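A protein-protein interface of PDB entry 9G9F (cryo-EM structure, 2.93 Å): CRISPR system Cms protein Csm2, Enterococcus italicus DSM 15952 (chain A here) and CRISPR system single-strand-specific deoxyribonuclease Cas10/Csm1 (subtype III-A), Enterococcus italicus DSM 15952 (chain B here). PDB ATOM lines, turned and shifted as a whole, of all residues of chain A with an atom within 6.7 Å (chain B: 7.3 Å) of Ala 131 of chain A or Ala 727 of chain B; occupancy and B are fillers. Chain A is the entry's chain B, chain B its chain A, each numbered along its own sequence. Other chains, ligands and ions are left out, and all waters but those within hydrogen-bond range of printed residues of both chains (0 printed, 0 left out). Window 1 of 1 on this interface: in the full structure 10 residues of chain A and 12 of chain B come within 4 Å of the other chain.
The guanidinium group of Arg 728 of chain B lies within salt-bridge range of the side-chain carboxylate of Glu 127 of chain A, 2.8 Å away.
The side-chain amino group of Lys 124 of chain A is in salt-bridge range of the side-chain carboxylate of Asp 722 of chain B, 3.7 Å away.
Of the printed residues of chain B, Ala 131 of chain A touches Ala 727.
Printed residues of chain B within 4 Å of Tyr 132 of chain A: Ala 727 and Phe 747.
Printed residues of chain B within 4 Å of Glu 127 of chain A: Ile 724 (3.6 Å) and Arg 728 (2.8 Å).
Asn 725 of chain B touches none of the printed residues of chain A.
Val 130 of chain A touches none of the printed residues of chain B.
The nearest printed residue of chain B that does not touch Leu 14 of chain A is Ala 727 of chain B (5.5 Å).
Among the printed residues, merely in contact across the chains: Leu 14 of chain A with Gln 723 of chain B (3.95 Å), Leu 14 of chain A with Ile 724 of chain B (3.5 Å), Lys 124 of chain A with Ile 724 of chain B (3.4 Å), Glu 127 of chain A with Ile 724 of chain B (3.6 Å), Ala 128 of chain A with Ile 724 of chain B (3.9 Å), Ala 131 of chain A with Ala 727 of chain B (3.3 Å), Tyr 132 of chain A with Ala 727 of chain B (3.7 Å), Tyr 132 of chain A with Phe 747 of chain B (3.7 Å), Lys 134 of chain A with Tyr 731 of chain B (3.3 Å), Lys 134 of chain A with Ala 734 of chain B (3.7 Å), Phe 135 of chain A with Ala 730 of chain B (3.6 Å), Phe 135 of chain A with Ala 734 of chain B (3.96 Å) and Phe 135 of chain A with Phe 747 of chain B (3.4 Å).
The backbone carbonyl oxygen (O) of Asp 722 of chain B sits close to the side-chain amide oxygen (OD1) of Asn 725 of chain B (3.2 Å).
The side-chain amide nitrogen (ND2) of Asn 725 of chain B lies close to the guanidinium group (NH1) of Arg 728 of chain B, 3.3 Å away.
Along chain A the printed residues that touch a printed residue of chain B span positions 14 to 135.
Printed residues of chain B that touch a printed residue of chain A: Asp 722, Gln 723, Ile 724, Ala 727, Arg 728, Ala 730, Tyr 731, Ala 734 and Phe 747.
Hydrophobic or aromatic side chains of chain B that line the printed part of chain A: Ile 724, Ala 727, Ala 730, Tyr 731, Ala 734 and Phe 747.
Among the printed residues, 15 pairs touch across the chains.
Among the printed residues, Asp or Glu carboxylates within 4 Å of a Lys or Arg side-chain nitrogen of the other chain: Lys 124 of chain A with Asp 722 of chain B (3.7 Å) and Glu 127 of chain A with Arg 728 of chain B (2.8 Å).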
ATOM      1  N   LEU A  14       7.973 -12.051 -28.524  1.00  0.00           N
ATOM      2  CA  LEU A  14       9.401 -11.762 -28.621  1.00  0.00           C
ATOM      3  C   LEU A  14       9.716 -10.991 -29.895  1.00  0.00           C
ATOM      4  O   LEU A  14      10.611 -10.134 -29.912  1.00  0.00           O
ATOM      5  CB  LEU A  14      10.200 -13.063 -28.559  1.00  0.00           C
ATOM      6  CG  LEU A  14      10.442 -13.723 -27.198  1.00  0.00           C
ATOM      7  CD1 LEU A  14       9.168 -13.941 -26.397  1.00  0.00           C
ATOM      8  CD2 LEU A  14      11.122 -15.041 -27.428  1.00  0.00           C
ATOM      9  N   LEU A  47      18.174  -1.002 -17.172  1.00  0.00           N
ATOM     10  CA  LEU A  47      17.548  -2.226 -17.654  1.00  0.00           C
ATOM     11  C   LEU A  47      18.063  -3.435 -16.888  1.00  0.00           C
ATOM     12  O   LEU A  47      17.303  -4.366 -16.600  1.00  0.00           O
ATOM     13  CB  LEU A  47      17.800  -2.384 -19.151  1.00  0.00           C
ATOM     14  CG  LEU A  47      17.278  -3.670 -19.780  1.00  0.00           C
ATOM     15  CD1 LEU A  47      15.798  -3.824 -19.503  1.00  0.00           C
ATOM     16  CD2 LEU A  47      17.550  -3.668 -21.268  1.00  0.00           C
ATOM     17  N   LEU A  51      15.937  -6.064 -14.737  1.00  0.00           N
ATOM     18  CA  LEU A  51      16.087  -7.497 -14.942  1.00  0.00           C
ATOM     19  C   LEU A  51      16.538  -8.203 -13.672  1.00  0.00           C
ATOM     20  O   LEU A  51      16.228  -9.380 -13.482  1.00  0.00           O
ATOM     21  CB  LEU A  51      17.073  -7.762 -16.075  1.00  0.00           C
ATOM     22  CG  LEU A  51      17.140  -9.214 -16.535  1.00  0.00           C
ATOM     23  CD1 LEU A  51      15.750  -9.758 -16.815  1.00  0.00           C
ATOM     24  CD2 LEU A  51      18.012  -9.317 -17.756  1.00  0.00           C
ATOM     25  N   LYS A 124      10.344 -14.252 -20.314  1.00  0.00           N
ATOM     26  CA  LYS A 124      10.984 -14.467 -21.609  1.00  0.00           C
ATOM     27  C   LYS A 124      10.967 -13.194 -22.443  1.00  0.00           C
ATOM     28  O   LYS A 124      11.958 -12.857 -23.096  1.00  0.00           O
ATOM     29  CB  LYS A 124      10.289 -15.601 -22.362  1.00  0.00           C
ATOM     30  CG  LYS A 124      10.382 -16.964 -21.698  1.00  0.00           C
ATOM     31  CD  LYS A 124       9.427 -17.949 -22.354  1.00  0.00           C
ATOM     32  CE  LYS A 124       9.292 -19.225 -21.541  1.00  0.00           C
ATOM     33  NZ  LYS A 124      10.584 -19.947 -21.420  1.00  0.00           N
ATOM     34  N   PHE A 126      10.844 -10.089 -21.295  1.00  0.00           N
ATOM     35  CA  PHE A 126      11.790  -9.145 -20.706  1.00  0.00           C
ATOM     36  C   PHE A 126      13.228  -9.497 -21.075  1.00  0.00           C
ATOM     37  O   PHE A 126      14.031  -8.616 -21.416  1.00  0.00           O
ATOM     38  CB  PHE A 126      11.622  -9.115 -19.191  1.00  0.00           C
ATOM     39  CG  PHE A 126      11.837  -7.762 -18.589  1.00  0.00           C
ATOM     40  CD1 PHE A 126      13.060  -7.132 -18.697  1.00  0.00           C
ATOM     41  CD2 PHE A 126      10.817  -7.122 -17.917  1.00  0.00           C
ATOM     42  CE1 PHE A 126      13.261  -5.890 -18.149  1.00  0.00           C
ATOM     43  CE2 PHE A 126      11.014  -5.881 -17.368  1.00  0.00           C
ATOM     44  CZ  PHE A 126      12.237  -5.264 -17.482  1.00  0.00           C
ATOM     45  N   GLU A 127      13.568 -10.783 -21.011  1.00  0.00           N
ATOM     46  CA  GLU A 127      14.916 -11.208 -21.364  1.00  0.00           C
ATOM     47  C   GLU A 127      15.202 -10.956 -22.839  1.00  0.00           C
ATOM     48  O   GLU A 127      16.322 -10.585 -23.208  1.00  0.00           O
ATOM     49  CB  GLU A 127      15.098 -12.681 -21.006  1.00  0.00           C
ATOM     50  CG  GLU A 127      16.304 -13.332 -21.626  1.00  0.00           C
ATOM     51  CD  GLU A 127      16.204 -14.839 -21.644  1.00  0.00           C
ATOM     52  OE1 GLU A 127      17.139 -15.483 -22.157  1.00  0.00           O
ATOM     53  OE2 GLU A 127      15.197 -15.381 -21.143  1.00  0.00           O
ATOM     54  N   ALA A 128      14.198 -11.148 -23.700  1.00  0.00           N
ATOM     55  CA  ALA A 128      14.360 -10.822 -25.112  1.00  0.00           C
ATOM     56  C   ALA A 128      14.600  -9.332 -25.307  1.00  0.00           C
ATOM     57  O   ALA A 128      15.431  -8.933 -26.132  1.00  0.00           O
ATOM     58  CB  ALA A 128      13.132 -11.273 -25.900  1.00  0.00           C
ATOM     59  N   LEU A 129      13.873  -8.496 -24.564  1.00  0.00           N
ATOM     60  CA  LEU A 129      14.109  -7.057 -24.622  1.00  0.00           C
ATOM     61  C   LEU A 129      15.553  -6.736 -24.274  1.00  0.00           C
ATOM     62  O   LEU A 129      16.218  -5.967 -24.977  1.00  0.00           O
ATOM     63  CB  LEU A 129      13.165  -6.326 -23.668  1.00  0.00           C
ATOM     64  CG  LEU A 129      11.780  -5.924 -24.164  1.00  0.00           C
ATOM     65  CD1 LEU A 129      11.049  -5.180 -23.070  1.00  0.00           C
ATOM     66  CD2 LEU A 129      11.884  -5.065 -25.404  1.00  0.00           C
ATOM     67  N   VAL A 130      16.059  -7.335 -23.195  1.00  0.00           N
ATOM     68  CA  VAL A 130      17.437  -7.075 -22.780  1.00  0.00           C
ATOM     69  C   VAL A 130      18.419  -7.537 -23.852  1.00  0.00           C
ATOM     70  O   VAL A 130      19.371  -6.820 -24.201  1.00  0.00           O
ATOM     71  CB  VAL A 130      17.721  -7.753 -21.428  1.00  0.00           C
ATOM     72  CG1 VAL A 130      19.161  -7.518 -21.012  1.00  0.00           C
ATOM     73  CG2 VAL A 130      16.764  -7.236 -20.375  1.00  0.00           C
ATOM     74  N   ALA A 131      18.202  -8.738 -24.392  1.00  0.00           N
ATOM     75  CA  ALA A 131      19.128  -9.300 -25.369  1.00  0.00           C
ATOM     76  C   ALA A 131      19.183  -8.449 -26.629  1.00  0.00           C
ATOM     77  O   ALA A 131      20.266  -8.124 -27.126  1.00  0.00           O
ATOM     78  CB  ALA A 131      18.719 -10.734 -25.706  1.00  0.00           C
ATOM     79  N   TYR A 132      18.019  -8.068 -27.156  1.00  0.00           N
ATOM     80  CA  TYR A 132      17.997  -7.267 -28.372  1.00  0.00           C
ATOM     81  C   TYR A 132      18.495  -5.853 -28.118  1.00  0.00           C
ATOM     82  O   TYR A 132      19.084  -5.239 -29.013  1.00  0.00           O
ATOM     83  CB  TYR A 132      16.588  -7.243 -28.958  1.00  0.00           C
ATOM     84  CG  TYR A 132      16.143  -8.581 -29.498  1.00  0.00           C
ATOM     85  CD1 TYR A 132      16.941  -9.300 -30.374  1.00  0.00           C
ATOM     86  CD2 TYR A 132      14.929  -9.131 -29.120  1.00  0.00           C
ATOM     87  CE1 TYR A 132      16.535 -10.522 -30.864  1.00  0.00           C
ATOM     88  CE2 TYR A 132      14.517 -10.351 -29.602  1.00  0.00           C
ATOM     89  CZ  TYR A 132      15.321 -11.041 -30.473  1.00  0.00           C
ATOM     90  OH  TYR A 132      14.901 -12.258 -30.952  1.00  0.00           O
ATOM     91  N   ALA A 133      18.277  -5.320 -26.913  1.00  0.00           N
ATOM     92  CA  ALA A 133      18.809  -4.004 -26.587  1.00  0.00           C
ATOM     93  C   ALA A 133      20.329  -4.014 -26.583  1.00  0.00           C
ATOM     94  O   ALA A 133      20.964  -3.068 -27.061  1.00  0.00           O
ATOM     95  CB  ALA A 133      18.267  -3.542 -25.237  1.00  0.00           C
ATOM     96  N   LYS A 134      20.934  -5.073 -26.041  1.00  0.00           N
ATOM     97  CA  LYS A 134      22.394  -5.155 -26.073  1.00  0.00           C
ATOM     98  C   LYS A 134      22.905  -5.431 -27.481  1.00  0.00           C
ATOM     99  O   LYS A 134      23.932  -4.880 -27.893  1.00  0.00           O
ATOM    100  CB  LYS A 134      22.895  -6.230 -25.114  1.00  0.00           C
ATOM    101  CG  LYS A 134      24.396  -6.459 -25.207  1.00  0.00           C
ATOM    102  CD  LYS A 134      25.175  -5.190 -24.912  1.00  0.00           C
ATOM    103  CE  LYS A 134      25.106  -4.837 -23.440  1.00  0.00           C
ATOM    104  NZ  LYS A 134      25.698  -5.910 -22.597  1.00  0.00           N
ATOM    105  N   PHE A 135      22.201  -6.281 -28.233  1.00  0.00           N
ATOM    106  CA  PHE A 135      22.675  -6.681 -29.553  1.00  0.00           C
ATOM    107  C   PHE A 135      22.762  -5.488 -30.497  1.00  0.00           C
ATOM    108  O   PHE A 135      23.739  -5.345 -31.240  1.00  0.00           O
ATOM    109  CB  PHE A 135      21.749  -7.755 -30.127  1.00  0.00           C
ATOM    110  CG  PHE A 135      22.115  -8.201 -31.514  1.00  0.00           C
ATOM    111  CD1 PHE A 135      23.442  -8.350 -31.887  1.00  0.00           C
ATOM    112  CD2 PHE A 135      21.130  -8.496 -32.438  1.00  0.00           C
ATOM    113  CE1 PHE A 135      23.776  -8.766 -33.158  1.00  0.00           C
ATOM    114  CE2 PHE A 135      21.459  -8.911 -33.711  1.00  0.00           C
ATOM    115  CZ  PHE A 135      22.783  -9.047 -34.071  1.00  0.00           C
ATOM    116  N   TYR A 136      21.758  -4.614 -30.471  1.00  0.00           N
ATOM    117  CA  TYR A 136      21.705  -3.512 -31.419  1.00  0.00           C
ATOM    118  C   TYR A 136      22.725  -2.423 -31.120  1.00  0.00           C
ATOM    119  O   TYR A 136      22.875  -1.505 -31.932  1.00  0.00           O
ATOM    120  CB  TYR A 136      20.296  -2.924 -31.449  1.00  0.00           C
ATOM    121  CG  TYR A 136      19.299  -3.799 -32.178  1.00  0.00           C
ATOM    122  CD1 TYR A 136      19.723  -4.763 -33.083  1.00  0.00           C
ATOM    123  CD2 TYR A 136      17.939  -3.665 -31.961  1.00  0.00           C
ATOM    124  CE1 TYR A 136      18.820  -5.566 -33.749  1.00  0.00           C
ATOM    125  CE2 TYR A 136      17.028  -4.464 -32.622  1.00  0.00           C
ATOM    126  CZ  TYR A 136      17.473  -5.411 -33.514  1.00  0.00           C
ATOM    127  OH  TYR A 136      16.565  -6.207 -34.171  1.00  0.00           O
ATOM    128  N   LEU B 717      22.618 -23.167 -28.404  1.00  0.00           N
ATOM    129  CA  LEU B 717      21.549 -22.211 -28.668  1.00  0.00           C
ATOM    130  C   LEU B 717      20.731 -22.618 -29.890  1.00  0.00           C
ATOM    131  O   LEU B 717      19.498 -22.535 -29.876  1.00  0.00           O
ATOM    132  CB  LEU B 717      22.132 -20.812 -28.863  1.00  0.00           C
ATOM    133  CG  LEU B 717      22.759 -20.154 -27.637  1.00  0.00           C
ATOM    134  CD1 LEU B 717      23.607 -18.974 -28.053  1.00  0.00           C
ATOM    135  CD2 LEU B 717      21.687 -19.729 -26.662  1.00  0.00           C
ATOM    136  N   ASP B 722      13.167 -23.547 -28.675  1.00  0.00           N
ATOM    137  CA  ASP B 722      12.449 -22.433 -28.075  1.00  0.00           C
ATOM    138  C   ASP B 722      12.858 -21.123 -28.734  1.00  0.00           C
ATOM    139  O   ASP B 722      14.029 -20.908 -29.057  1.00  0.00           O
ATOM    140  CB  ASP B 722      12.708 -22.374 -26.570  1.00  0.00           C
ATOM    141  CG  ASP B 722      11.591 -21.676 -25.814  1.00  0.00           C
ATOM    142  OD1 ASP B 722      10.560 -21.350 -26.440  1.00  0.00           O
ATOM    143  OD2 ASP B 722      11.741 -21.453 -24.594  1.00  0.00           O
ATOM    144  N   GLN B 723      11.882 -20.244 -28.974  1.00  0.00           N
ATOM    145  CA  GLN B 723      12.178 -18.985 -29.708  1.00  0.00           C
ATOM    146  C   GLN B 723      13.143 -18.100 -28.911  1.00  0.00           C
ATOM    147  O   GLN B 723      14.012 -17.462 -29.537  1.00  0.00           O
ATOM    148  CB  GLN B 723      10.886 -18.207 -29.944  1.00  0.00           C
ATOM    149  CG  GLN B 723       9.736 -19.060 -30.469  1.00  0.00           C
ATOM    150  CD  GLN B 723       8.430 -18.302 -30.550  1.00  0.00           C
ATOM    151  OE1 GLN B 723       7.920 -17.787 -29.549  1.00  0.00           O
ATOM    152  NE2 GLN B 723       7.877 -18.220 -31.751  1.00  0.00           N
ATOM    153  N   ILE B 724      12.998 -18.054 -27.589  1.00  0.00           N
ATOM    154  CA  ILE B 724      13.819 -17.142 -26.798  1.00  0.00           C
ATOM    155  C   ILE B 724      15.298 -17.371 -27.057  1.00  0.00           C
ATOM    156  O   ILE B 724      16.101 -16.431 -26.992  1.00  0.00           O
ATOM    157  CB  ILE B 724      13.469 -17.284 -25.302  1.00  0.00           C
ATOM    158  CG1 ILE B 724      14.321 -16.340 -24.452  1.00  0.00           C
ATOM    159  CG2 ILE B 724      13.631 -18.723 -24.847  1.00  0.00           C
ATOM    160  CD1 ILE B 724      14.149 -14.880 -24.802  1.00  0.00           C
ATOM    161  N   ASN B 725      15.678 -18.607 -27.391  1.00  0.00           N
ATOM    162  CA  ASN B 725      17.082 -18.914 -27.634  1.00  0.00           C
ATOM    163  C   ASN B 725      17.667 -18.014 -28.710  1.00  0.00           C
ATOM    164  O   ASN B 725      18.820 -17.581 -28.600  1.00  0.00           O
ATOM    165  CB  ASN B 725      17.239 -20.382 -28.014  1.00  0.00           C
ATOM    166  CG  ASN B 725      17.002 -21.310 -26.845  1.00  0.00           C
ATOM    167  OD1 ASN B 725      15.866 -21.680 -26.554  1.00  0.00           O
ATOM    168  ND2 ASN B 725      18.076 -21.689 -26.163  1.00  0.00           N
ATOM    169  N   ILE B 726      16.879 -17.688 -29.738  1.00  0.00           N
ATOM    170  CA  ILE B 726      17.369 -16.790 -30.782  1.00  0.00           C
ATOM    171  C   ILE B 726      17.850 -15.487 -30.161  1.00  0.00           C
ATOM    172  O   ILE B 726      18.977 -15.038 -30.407  1.00  0.00           O
ATOM    173  CB  ILE B 726      16.278 -16.536 -31.836  1.00  0.00           C
ATOM    174  CG1 ILE B 726      15.777 -17.855 -32.424  1.00  0.00           C
ATOM    175  CG2 ILE B 726      16.806 -15.619 -32.928  1.00  0.00           C
ATOM    176  CD1 ILE B 726      14.306 -17.845 -32.775  1.00  0.00           C
ATOM    177  N   ALA B 727      17.021 -14.895 -29.298  1.00  0.00           N
ATOM    178  CA  ALA B 727      17.419 -13.678 -28.601  1.00  0.00           C
ATOM    179  C   ALA B 727      18.702 -13.903 -27.817  1.00  0.00           C
ATOM    180  O   ALA B 727      19.632 -13.091 -27.881  1.00  0.00           O
ATOM    181  CB  ALA B 727      16.295 -13.212 -27.678  1.00  0.00           C
ATOM    182  N   ARG B 728      18.783 -15.029 -27.101  1.00  0.00           N
ATOM    183  CA  ARG B 728      20.001 -15.343 -26.367  1.00  0.00           C
ATOM    184  C   ARG B 728      21.193 -15.367 -27.307  1.00  0.00           C
ATOM    185  O   ARG B 728      22.250 -14.803 -26.999  1.00  0.00           O
ATOM    186  CB  ARG B 728      19.850 -16.683 -25.650  1.00  0.00           C
ATOM    187  CG  ARG B 728      18.810 -16.677 -24.551  1.00  0.00           C
ATOM    188  CD  ARG B 728      18.450 -18.085 -24.113  1.00  0.00           C
ATOM    189  NE  ARG B 728      17.370 -18.089 -23.135  1.00  0.00           N
ATOM    190  CZ  ARG B 728      16.663 -19.158 -22.798  1.00  0.00           C
ATOM    191  NH1 ARG B 728      16.892 -20.340 -23.346  1.00  0.00           N
ATOM    192  NH2 ARG B 728      15.699 -19.039 -21.891  1.00  0.00           N
ATOM    193  N   LEU B 729      21.018 -15.975 -28.482  1.00  0.00           N
ATOM    194  CA  LEU B 729      22.078 -15.993 -29.479  1.00  0.00           C
ATOM    195  C   LEU B 729      22.537 -14.578 -29.781  1.00  0.00           C
ATOM    196  O   LEU B 729      23.738 -14.284 -29.760  1.00  0.00           O
ATOM    197  CB  LEU B 729      21.584 -16.695 -30.745  1.00  0.00           C
ATOM    198  CG  LEU B 729      22.593 -17.043 -31.835  1.00  0.00           C
ATOM    199  CD1 LEU B 729      22.283 -18.414 -32.396  1.00  0.00           C
ATOM    200  CD2 LEU B 729      22.564 -16.005 -32.936  1.00  0.00           C
ATOM    201  N   ALA B 730      21.580 -13.671 -30.000  1.00  0.00           N
ATOM    202  CA  ALA B 730      21.918 -12.273 -30.231  1.00  0.00           C
ATOM    203  C   ALA B 730      22.818 -11.749 -29.124  1.00  0.00           C
ATOM    204  O   ALA B 730      23.891 -11.193 -29.392  1.00  0.00           O
ATOM    205  CB  ALA B 730      20.644 -11.437 -30.337  1.00  0.00           C
ATOM    206  N   TYR B 731      22.426 -11.979 -27.865  1.00  0.00           N
ATOM    207  CA  TYR B 731      23.244 -11.505 -26.755  1.00  0.00           C
ATOM    208  C   TYR B 731      24.656 -12.048 -26.862  1.00  0.00           C
ATOM    209  O   TYR B 731      25.631 -11.301 -26.711  1.00  0.00           O
ATOM    210  CB  TYR B 731      22.649 -11.927 -25.416  1.00  0.00           C
ATOM    211  CG  TYR B 731      23.252 -11.177 -24.250  1.00  0.00           C
ATOM    212  CD1 TYR B 731      23.437  -9.806 -24.304  1.00  0.00           C
ATOM    213  CD2 TYR B 731      23.752 -11.855 -23.154  1.00  0.00           C
ATOM    214  CE1 TYR B 731      24.007  -9.125 -23.247  1.00  0.00           C
ATOM    215  CE2 TYR B 731      24.321 -11.184 -22.094  1.00  0.00           C
ATOM    216  CZ  TYR B 731      24.455  -9.820 -22.149  1.00  0.00           C
ATOM    217  OH  TYR B 731      25.034  -9.143 -21.103  1.00  0.00           O
ATOM    218  N   LEU B 732      24.785 -13.347 -27.140  1.00  0.00           N
ATOM    219  CA  LEU B 732      26.109 -13.934 -27.276  1.00  0.00           C
ATOM    220  C   LEU B 732      26.876 -13.229 -28.383  1.00  0.00           C
ATOM    221  O   LEU B 732      28.017 -12.790 -28.190  1.00  0.00           O
ATOM    222  CB  LEU B 732      25.982 -15.431 -27.555  1.00  0.00           C
ATOM    223  CG  LEU B 732      27.233 -16.282 -27.789  1.00  0.00           C
ATOM    224  CD1 LEU B 732      28.420 -15.784 -26.975  1.00  0.00           C
ATOM    225  CD2 LEU B 732      26.940 -17.735 -27.468  1.00  0.00           C
ATOM    226  N   LEU B 733      26.220 -13.032 -29.527  1.00  0.00           N
ATOM    227  CA  LEU B 733      26.869 -12.382 -30.652  1.00  0.00           C
ATOM    228  C   LEU B 733      27.216 -10.937 -30.335  1.00  0.00           C
ATOM    229  O   LEU B 733      28.053 -10.344 -31.023  1.00  0.00           O
ATOM    230  CB  LEU B 733      25.966 -12.466 -31.885  1.00  0.00           C
ATOM    231  CG  LEU B 733      26.142 -13.676 -32.811  1.00  0.00           C
ATOM    232  CD1 LEU B 733      25.939 -14.987 -32.070  1.00  0.00           C
ATOM    233  CD2 LEU B 733      25.186 -13.585 -33.984  1.00  0.00           C
ATOM    234  N   ALA B 734      26.598 -10.364 -29.300  1.00  0.00           N
ATOM    235  CA  ALA B 734      26.943  -9.008 -28.894  1.00  0.00           C
ATOM    236  C   ALA B 734      28.299  -8.969 -28.204  1.00  0.00           C
ATOM    237  O   ALA B 734      29.069  -8.020 -28.390  1.00  0.00           O
ATOM    238  CB  ALA B 734      25.857  -8.442 -27.981  1.00  0.00           C
ATOM    239  N   PHE B 747      23.105 -14.273 -37.375  1.00  0.00           N
ATOM    240  CA  PHE B 747      21.770 -13.935 -36.892  1.00  0.00           C
ATOM    241  C   PHE B 747      20.714 -14.231 -37.951  1.00  0.00           C
ATOM    242  O   PHE B 747      19.673 -14.837 -37.662  1.00  0.00           O
ATOM    243  CB  PHE B 747      21.733 -12.465 -36.478  1.00  0.00           C
ATOM    244  CG  PHE B 747      20.584 -12.114 -35.581  1.00  0.00           C
ATOM    245  CD1 PHE B 747      20.311 -12.872 -34.458  1.00  0.00           C
ATOM    246  CD2 PHE B 747      19.786 -11.020 -35.855  1.00  0.00           C
ATOM    247  CE1 PHE B 747      19.258 -12.550 -33.631  1.00  0.00           C
ATOM    248  CE2 PHE B 747      18.733 -10.693 -35.031  1.00  0.00           C
ATOM    249  CZ  PHE B 747      18.469 -11.458 -33.917  1.00  0.00           C
ATOM    250  N   GLN B 751      17.647 -17.006 -37.756  1.00  0.00           N
ATOM    251  CA  GLN B 751      16.235 -16.647 -37.872  1.00  0.00           C
ATOM    252  C   GLN B 751      15.478 -17.615 -38.777  1.00  0.00           C
ATOM    253  O   GLN B 751      14.387 -18.079 -38.424  1.00  0.00           O
ATOM    254  CB  GLN B 751      16.096 -15.214 -38.384  1.00  0.00           C
ATOM    255  CG  GLN B 751      16.677 -14.176 -37.451  1.00  0.00           C
ATOM    256  CD  GLN B 751      15.708 -13.773 -36.365  1.00  0.00           C
ATOM    257  OE1 GLN B 751      14.561 -14.221 -36.342  1.00  0.00           O
ATOM    258  NE2 GLN B 751      16.162 -12.924 -35.453  1.00  0.00           N
